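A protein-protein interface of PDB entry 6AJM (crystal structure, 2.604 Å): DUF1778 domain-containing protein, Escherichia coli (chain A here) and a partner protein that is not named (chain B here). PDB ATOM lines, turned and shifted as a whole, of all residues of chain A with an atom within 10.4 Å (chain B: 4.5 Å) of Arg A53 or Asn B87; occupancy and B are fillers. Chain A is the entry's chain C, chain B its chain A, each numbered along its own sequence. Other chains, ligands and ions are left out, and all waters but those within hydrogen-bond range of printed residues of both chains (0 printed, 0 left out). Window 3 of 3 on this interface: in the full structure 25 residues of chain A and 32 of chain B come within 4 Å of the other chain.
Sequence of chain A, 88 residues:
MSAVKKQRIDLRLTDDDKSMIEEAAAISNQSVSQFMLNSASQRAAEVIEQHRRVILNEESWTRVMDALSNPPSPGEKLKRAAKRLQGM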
ATOM      1  N   ALA A  45     -12.645 -10.905   3.049  1.00  0.00           N
ATOM      2  CA  ALA A  45     -13.014 -12.315   3.116  1.00  0.00           C
ATOM      3  C   ALA A  45     -14.532 -12.495   3.179  1.00  0.00           C
ATOM      4  O   ALA A  45     -15.098 -13.323   2.453  1.00  0.00           O
ATOM      5  CB  ALA A  45     -12.332 -12.982   4.305  1.00  0.00           C
ATOM      6  N   GLU A  46     -15.225 -11.713   4.016  1.00  0.00           N
ATOM      7  CA  GLU A  46     -16.659 -11.985   4.096  1.00  0.00           C
ATOM      8  C   GLU A  46     -17.414 -11.450   2.875  1.00  0.00           C
ATOM      9  O   GLU A  46     -18.420 -12.044   2.468  1.00  0.00           O
ATOM     10  CB  GLU A  46     -17.257 -11.482   5.421  1.00  0.00           C
ATOM     11  CG  GLU A  46     -17.231 -10.011   5.732  1.00  0.00           C
ATOM     12  CD  GLU A  46     -17.746  -9.724   7.151  1.00  0.00           C
ATOM     13  OE1 GLU A  46     -17.302 -10.414   8.100  1.00  0.00           O
ATOM     14  OE2 GLU A  46     -18.600  -8.824   7.320  1.00  0.00           O
ATOM     15  N   VAL A  47     -16.926 -10.380   2.240  1.00  0.00           N
ATOM     16  CA  VAL A  47     -17.561  -9.911   1.012  1.00  0.00           C
ATOM     17  C   VAL A  47     -17.449 -10.979  -0.072  1.00  0.00           C
ATOM     18  O   VAL A  47     -18.422 -11.276  -0.782  1.00  0.00           O
ATOM     19  CB  VAL A  47     -16.957  -8.567   0.552  1.00  0.00           C
ATOM     20  CG1 VAL A  47     -17.335  -8.295  -0.870  1.00  0.00           C
ATOM     21  CG2 VAL A  47     -17.463  -7.415   1.403  1.00  0.00           C
ATOM     22  N   ILE A  48     -16.267 -11.594  -0.200  1.00  0.00           N
ATOM     23  CA  ILE A  48     -16.100 -12.637  -1.207  1.00  0.00           C
ATOM     24  C   ILE A  48     -16.959 -13.849  -0.878  1.00  0.00           C
ATOM     25  O   ILE A  48     -17.670 -14.380  -1.741  1.00  0.00           O
ATOM     26  CB  ILE A  48     -14.623 -13.021  -1.338  1.00  0.00           C
ATOM     27  CG1 ILE A  48     -13.828 -11.863  -1.936  1.00  0.00           C
ATOM     28  CG2 ILE A  48     -14.492 -14.262  -2.192  1.00  0.00           C
ATOM     29  CD1 ILE A  48     -12.339 -11.981  -1.679  1.00  0.00           C
ATOM     30  N   GLU A  49     -16.930 -14.300   0.377  1.00  0.00           N
ATOM     31  CA  GLU A  49     -17.765 -15.438   0.741  1.00  0.00           C
ATOM     32  C   GLU A  49     -19.233 -15.157   0.431  1.00  0.00           C
ATOM     33  O   GLU A  49     -19.919 -16.002  -0.151  1.00  0.00           O
ATOM     34  CB  GLU A  49     -17.557 -15.813   2.217  1.00  0.00           C
ATOM     35  CG  GLU A  49     -16.618 -17.029   2.459  1.00  0.00           C
ATOM     36  CD  GLU A  49     -16.092 -17.150   3.922  1.00  0.00           C
ATOM     37  OE1 GLU A  49     -16.377 -16.257   4.756  1.00  0.00           O
ATOM     38  OE2 GLU A  49     -15.385 -18.145   4.236  1.00  0.00           O
ATOM     39  N   GLN A  50     -19.725 -13.953   0.755  1.00  0.00           N
ATOM     40  CA  GLN A  50     -21.148 -13.694   0.575  1.00  0.00           C
ATOM     41  C   GLN A  50     -21.507 -13.497  -0.891  1.00  0.00           C
ATOM     42  O   GLN A  50     -22.638 -13.796  -1.291  1.00  0.00           O
ATOM     43  CB  GLN A  50     -21.580 -12.486   1.408  1.00  0.00           C
ATOM     44  CG  GLN A  50     -23.088 -12.275   1.394  1.00  0.00           C
ATOM     45  CD  GLN A  50     -23.531 -11.056   2.180  1.00  0.00           C
ATOM     46  OE1 GLN A  50     -22.934 -10.709   3.208  1.00  0.00           O
ATOM     47  NE2 GLN A  50     -24.583 -10.392   1.695  1.00  0.00           N
ATOM     48  N   HIS A  51     -20.563 -13.012  -1.701  1.00  0.00           N
ATOM     49  CA  HIS A  51     -20.793 -12.856  -3.137  1.00  0.00           C
ATOM     50  C   HIS A  51     -20.898 -14.205  -3.838  1.00  0.00           C
ATOM     51  O   HIS A  51     -21.750 -14.384  -4.716  1.00  0.00           O
ATOM     52  CB  HIS A  51     -19.659 -12.035  -3.752  1.00  0.00           C
ATOM     53  CG  HIS A  51     -19.710 -11.946  -5.243  1.00  0.00           C
ATOM     54  ND1 HIS A  51     -20.442 -10.984  -5.908  1.00  0.00           N
ATOM     55  CD2 HIS A  51     -19.111 -12.690  -6.202  1.00  0.00           C
ATOM     56  CE1 HIS A  51     -20.294 -11.143  -7.212  1.00  0.00           C
ATOM     57  NE2 HIS A  51     -19.490 -12.170  -7.417  1.00  0.00           N
ATOM     58  N   ARG A  52     -20.030 -15.162  -3.477  1.00  0.00           N
ATOM     59  CA  ARG A  52     -20.038 -16.467  -4.148  1.00  0.00           C
ATOM     60  C   ARG A  52     -21.222 -17.357  -3.743  1.00  0.00           C
ATOM     61  O   ARG A  52     -21.558 -18.287  -4.483  1.00  0.00           O
ATOM     62  CB  ARG A  52     -18.743 -17.244  -3.877  1.00  0.00           C
ATOM     63  CG  ARG A  52     -17.407 -16.595  -4.291  1.00  0.00           C
ATOM     64  CD  ARG A  52     -16.342 -17.650  -4.121  1.00  0.00           C
ATOM     65  NE  ARG A  52     -14.961 -17.209  -3.929  1.00  0.00           N
ATOM     66  CZ  ARG A  52     -14.304 -16.446  -4.788  1.00  0.00           C
ATOM     67  NH1 ARG A  52     -14.951 -15.985  -5.846  1.00  0.00           N
ATOM     68  NH2 ARG A  52     -13.038 -16.116  -4.590  1.00  0.00           N
ATOM     69  N   ARG A  53     -21.847 -17.120  -2.589  1.00  0.00           N
ATOM     70  CA  ARG A  53     -22.883 -18.007  -2.062  1.00  0.00           C
ATOM     71  C   ARG A  53     -24.271 -17.600  -2.540  1.00  0.00           C
ATOM     72  O   ARG A  53     -24.571 -16.417  -2.699  1.00  0.00           O
ATOM     73  CB  ARG A  53     -22.890 -17.994  -0.536  1.00  0.00           C
ATOM     74  CG  ARG A  53     -21.961 -18.975   0.119  1.00  0.00           C
ATOM     75  CD  ARG A  53     -22.104 -18.932   1.632  1.00  0.00           C
ATOM     76  NE  ARG A  53     -21.587 -20.172   2.200  1.00  0.00           N
ATOM     77  CZ  ARG A  53     -22.299 -21.293   2.298  1.00  0.00           C
ATOM     78  NH1 ARG A  53     -23.562 -21.316   1.878  1.00  0.00           N
ATOM     79  NH2 ARG A  53     -21.755 -22.388   2.815  1.00  0.00           N
ATOM     80  N   VAL A  54     -25.125 -18.599  -2.761  1.00  0.00           N
ATOM     81  CA  VAL A  54     -26.540 -18.372  -3.044  1.00  0.00           C
ATOM     82  C   VAL A  54     -27.327 -19.029  -1.925  1.00  0.00           C
ATOM     83  O   VAL A  54     -27.198 -20.236  -1.697  1.00  0.00           O
ATOM     84  CB  VAL A  54     -26.992 -18.939  -4.399  1.00  0.00           C
ATOM     85  CG1 VAL A  54     -28.341 -18.334  -4.769  1.00  0.00           C
ATOM     86  CG2 VAL A  54     -25.984 -18.686  -5.478  1.00  0.00           C
ATOM     87  N   ILE A  55     -28.137 -18.252  -1.230  1.00  0.00           N
ATOM     88  CA  ILE A  55     -29.014 -18.797  -0.207  1.00  0.00           C
ATOM     89  C   ILE A  55     -30.396 -18.973  -0.815  1.00  0.00           C
ATOM     90  O   ILE A  55     -30.926 -18.053  -1.442  1.00  0.00           O
ATOM     91  CB  ILE A  55     -29.044 -17.899   1.036  1.00  0.00           C
ATOM     92  CG1 ILE A  55     -27.606 -17.631   1.500  1.00  0.00           C
ATOM     93  CG2 ILE A  55     -29.896 -18.550   2.120  1.00  0.00           C
ATOM     94  CD1 ILE A  55     -27.328 -17.973   2.946  1.00  0.00           C
ATOM     95  N   LEU A  56     -30.953 -20.173  -0.683  1.00  0.00           N
ATOM     96  CA  LEU A  56     -32.212 -20.535  -1.314  1.00  0.00           C
ATOM     97  C   LEU A  56     -33.264 -20.701  -0.238  1.00  0.00           C
ATOM     98  O   LEU A  56     -33.039 -21.409   0.748  1.00  0.00           O
ATOM     99  CB  LEU A  56     -32.078 -21.824  -2.124  1.00  0.00           C
ATOM    100  CG  LEU A  56     -30.995 -21.831  -3.221  1.00  0.00           C
ATOM    101  CD1 LEU A  56     -30.965 -23.160  -3.993  1.00  0.00           C
ATOM    102  CD2 LEU A  56     -31.187 -20.702  -4.172  1.00  0.00           C
ATOM    103  N   TRP A  61     -35.189 -23.906  -2.991  1.00  0.00           N
ATOM    104  CA  TRP A  61     -34.473 -25.133  -2.667  1.00  0.00           C
ATOM    105  C   TRP A  61     -35.229 -26.344  -3.177  1.00  0.00           C
ATOM    106  O   TRP A  61     -34.639 -27.243  -3.783  1.00  0.00           O
ATOM    107  CB  TRP A  61     -34.266 -25.244  -1.155  1.00  0.00           C
ATOM    108  CG  TRP A  61     -33.600 -26.534  -0.705  1.00  0.00           C
ATOM    109  CD1 TRP A  61     -34.215 -27.651  -0.206  1.00  0.00           C
ATOM    110  CD2 TRP A  61     -32.194 -26.820  -0.711  1.00  0.00           C
ATOM    111  NE1 TRP A  61     -33.277 -28.611   0.096  1.00  0.00           N
ATOM    112  CE2 TRP A  61     -32.030 -28.126  -0.204  1.00  0.00           C
ATOM    113  CE3 TRP A  61     -31.062 -26.097  -1.093  1.00  0.00           C
ATOM    114  CZ2 TRP A  61     -30.777 -28.719  -0.068  1.00  0.00           C
ATOM    115  CZ3 TRP A  61     -29.838 -26.679  -0.971  1.00  0.00           C
ATOM    116  CH2 TRP A  61     -29.697 -27.980  -0.453  1.00  0.00           C
ATOM    117  N   CYS B  68     -21.844 -21.496  -5.231  1.00  0.00           N
ATOM    118  CA  CYS B  68     -22.320 -22.590  -4.411  1.00  0.00           C
ATOM    119  C   CYS B  68     -23.617 -22.135  -3.762  1.00  0.00           C
ATOM    120  O   CYS B  68     -23.869 -20.935  -3.628  1.00  0.00           O
ATOM    121  CB  CYS B  68     -21.252 -23.018  -3.381  1.00  0.00           C
ATOM    122  SG  CYS B  68     -20.595 -21.693  -2.360  1.00  0.00           S
ATOM    123  N   GLU B  70     -26.993 -23.066  -0.738  1.00  0.00           N
ATOM    124  CA  GLU B  70     -27.358 -23.614   0.558  1.00  0.00           C
ATOM    125  C   GLU B  70     -28.837 -23.355   0.800  1.00  0.00           C
ATOM    126  O   GLU B  70     -29.450 -22.516   0.138  1.00  0.00           O
ATOM    127  CB  GLU B  70     -26.515 -23.002   1.682  1.00  0.00           C
ATOM    128  CG  GLU B  70     -26.392 -23.917   2.907  1.00  0.00           C
ATOM    129  CD  GLU B  70     -25.571 -23.305   4.026  1.00  0.00           C
ATOM    130  OE1 GLU B  70     -25.265 -22.090   3.927  1.00  0.00           O
ATOM    131  OE2 GLU B  70     -25.237 -24.039   4.991  1.00  0.00           O
ATOM    132  N   TYR B  85     -23.683 -30.416   4.710  1.00  0.00           N
ATOM    133  CA  TYR B  85     -23.215 -30.202   3.339  1.00  0.00           C
ATOM    134  C   TYR B  85     -23.321 -28.697   3.101  1.00  0.00           C
ATOM    135  O   TYR B  85     -24.390 -28.190   2.748  1.00  0.00           O
ATOM    136  CB  TYR B  85     -24.054 -31.003   2.349  1.00  0.00           C
ATOM    137  CG  TYR B  85     -23.407 -31.250   1.001  1.00  0.00           C
ATOM    138  CD1 TYR B  85     -22.193 -30.663   0.662  1.00  0.00           C
ATOM    139  CD2 TYR B  85     -24.017 -32.073   0.059  1.00  0.00           C
ATOM    140  CE1 TYR B  85     -21.602 -30.892  -0.583  1.00  0.00           C
ATOM    141  CE2 TYR B  85     -23.436 -32.305  -1.184  1.00  0.00           C
ATOM    142  CZ  TYR B  85     -22.230 -31.713  -1.500  1.00  0.00           C
ATOM    143  OH  TYR B  85     -21.657 -31.949  -2.729  1.00  0.00           O
ATOM    144  N   LYS B  86     -22.213 -27.986   3.304  1.00  0.00           N
ATOM    145  CA  LYS B  86     -22.278 -26.548   3.517  1.00  0.00           C
ATOM    146  C   LYS B  86     -21.907 -25.708   2.300  1.00  0.00           C
ATOM    147  O   LYS B  86     -22.252 -24.520   2.274  1.00  0.00           O
ATOM    148  CB  LYS B  86     -21.371 -26.157   4.695  1.00  0.00           C
ATOM    149  CG  LYS B  86     -21.778 -26.767   6.042  1.00  0.00           C
ATOM    150  CD  LYS B  86     -23.032 -26.108   6.626  1.00  0.00           C
ATOM    151  CE  LYS B  86     -23.497 -26.793   7.914  1.00  0.00           C
ATOM    152  NZ  LYS B  86     -22.469 -26.787   8.995  1.00  0.00           N
ATOM    153  N   ASN B  87     -21.242 -26.276   1.290  1.00  0.00           N
ATOM    154  CA  ASN B  87     -20.695 -25.500   0.166  1.00  0.00           C
ATOM    155  C   ASN B  87     -21.051 -26.124  -1.183  1.00  0.00           C
ATOM    156  O   ASN B  87     -20.177 -26.387  -2.011  1.00  0.00           O
ATOM    157  CB  ASN B  87     -19.179 -25.347   0.285  1.00  0.00           C
ATOM    158  CG  ASN B  87     -18.771 -24.110   1.067  1.00  0.00           C
ATOM    159  OD1 ASN B  87     -19.382 -23.050   0.934  1.00  0.00           O
ATOM    160  ND2 ASN B  87     -17.725 -24.241   1.884  1.00  0.00           N
ATOM    161  N   ILE B  88     -22.333 -26.401  -1.417  1.00  0.00           N
ATOM    162  CA  ILE B  88     -22.773 -27.188  -2.578  1.00  0.00           C
ATOM    163  C   ILE B  88     -22.376 -26.538  -3.900  1.00  0.00           C
ATOM    164  O   ILE B  88     -22.888 -25.460  -4.229  1.00  0.00           O
ATOM    165  CB  ILE B  88     -24.290 -27.424  -2.563  1.00  0.00           C
ATOM    166  CG1 ILE B  88     -24.762 -27.920  -1.196  1.00  0.00           C
ATOM    167  CG2 ILE B  88     -24.649 -28.434  -3.644  1.00  0.00           C
ATOM    168  CD1 ILE B  88     -26.283 -28.005  -1.078  1.00  0.00           C
ATOM    169  N   PRO B  89     -21.535 -27.186  -4.710  1.00  0.00           N
ATOM    170  CA  PRO B  89     -20.877 -26.487  -5.832  1.00  0.00           C
ATOM    171  C   PRO B  89     -21.727 -26.393  -7.080  1.00  0.00           C
ATOM    172  O   PRO B  89     -22.369 -27.357  -7.509  1.00  0.00           O
ATOM    173  CB  PRO B  89     -19.630 -27.334  -6.102  1.00  0.00           C
ATOM    174  CG  PRO B  89     -19.980 -28.726  -5.562  1.00  0.00           C
ATOM    175  CD  PRO B  89     -20.965 -28.522  -4.433  1.00  0.00           C
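Hydrophobic or aromatic side chains of chain A that line the printed part of chain B: Val A54, Leu A56 and Trp A61. Of the 7 printed residues of chain B, 5 touch a printed residue of chain A. Printed residues of chain B that touch a printed residue of chain A: Cys B68, Glu B70, Lys B86, Asn B87 and Ile B88. Hydrophobic or aromatic side chains of chain B within 4 Å of the printed part of chain A: Ile B88. Along chain B the printed residues that touch a printed residue of chain A span positions 68 to 88. Among the printed residues, Asp or Glu carboxylates within 4 Å of a Lys or Arg side-chain nitrogen of the other chain: Arg A53 with Glu B70 (2.8 Å).
Glu A46 touches none of the printed residues of chain B. Val A47 touches none of the printed residues of chain B. Of the printed residues of chain B, Arg A52 touches Cys B68. Printed residues of chain B within 4 Å of Val A54: Cys B68 (2.8 Å) and Glu B70 (3.0 Å). Printed residues of chain B within 4 Å of Leu A56: Glu B70 (2.9 Å). Printed residues of chain B within 4 Å of Trp A61: Glu B70 and Ile B88. Of the printed residues of chain A, Cys B68 touches Arg A52 (3.3 Å), Arg A53 (3.5 Å) and Val A54 (2.8 Å). Of chain A, only Arg A53 (2.8 Å), Val A54 (3.0 Å), Ile A55 (3.8 Å), Leu A56 (2.9 Å) and Trp A61 (3.9 Å) come within 4 Å of Glu B70. Printed residues of chain A within 4 Å of Lys B86: Arg A53. Of chain A, only Arg A53 comes within 4 Å of Asn B87.
The side-chain sulfur (SG) of Cys B68 lies within hydrogen-bond range of the side-chain amide oxygen (OD1) of Asn B87, 3.8 Å away.
The backbone NH (N) of Cys B68 is in hydrogen-bond range of the backbone carbonyl oxygen (O) of Arg A52 (3.3 Å). N of Val A54 is in hydrogen-bond range of O of Cys B68, at 2.8 Å. NH1 of Arg A53 is in salt-bridge range of OE1 of Glu B70 (2.8 Å). N of Glu B70 is in hydrogen-bond range of O of Val A54, at 3.0 Å. N of Leu A56 is in hydrogen-bond range of O of Glu B70, 2.9 Å away. The backbone carbonyl oxygen (O) of Lys B86 lies close to the guanidinium group (NH1) of Arg A53, 3.5 Å away. The guanidinium group of Arg A53 is in hydrogen-bond range of the side-chain amide oxygen of Asn B87, at 3.1 Å.
Arg A53 touches Cys B68 (CA to O, 3.5 Å). Ile A55 touches Glu B70. Glu B70 touches Trp A61. Ile B88 touches Trp A61.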
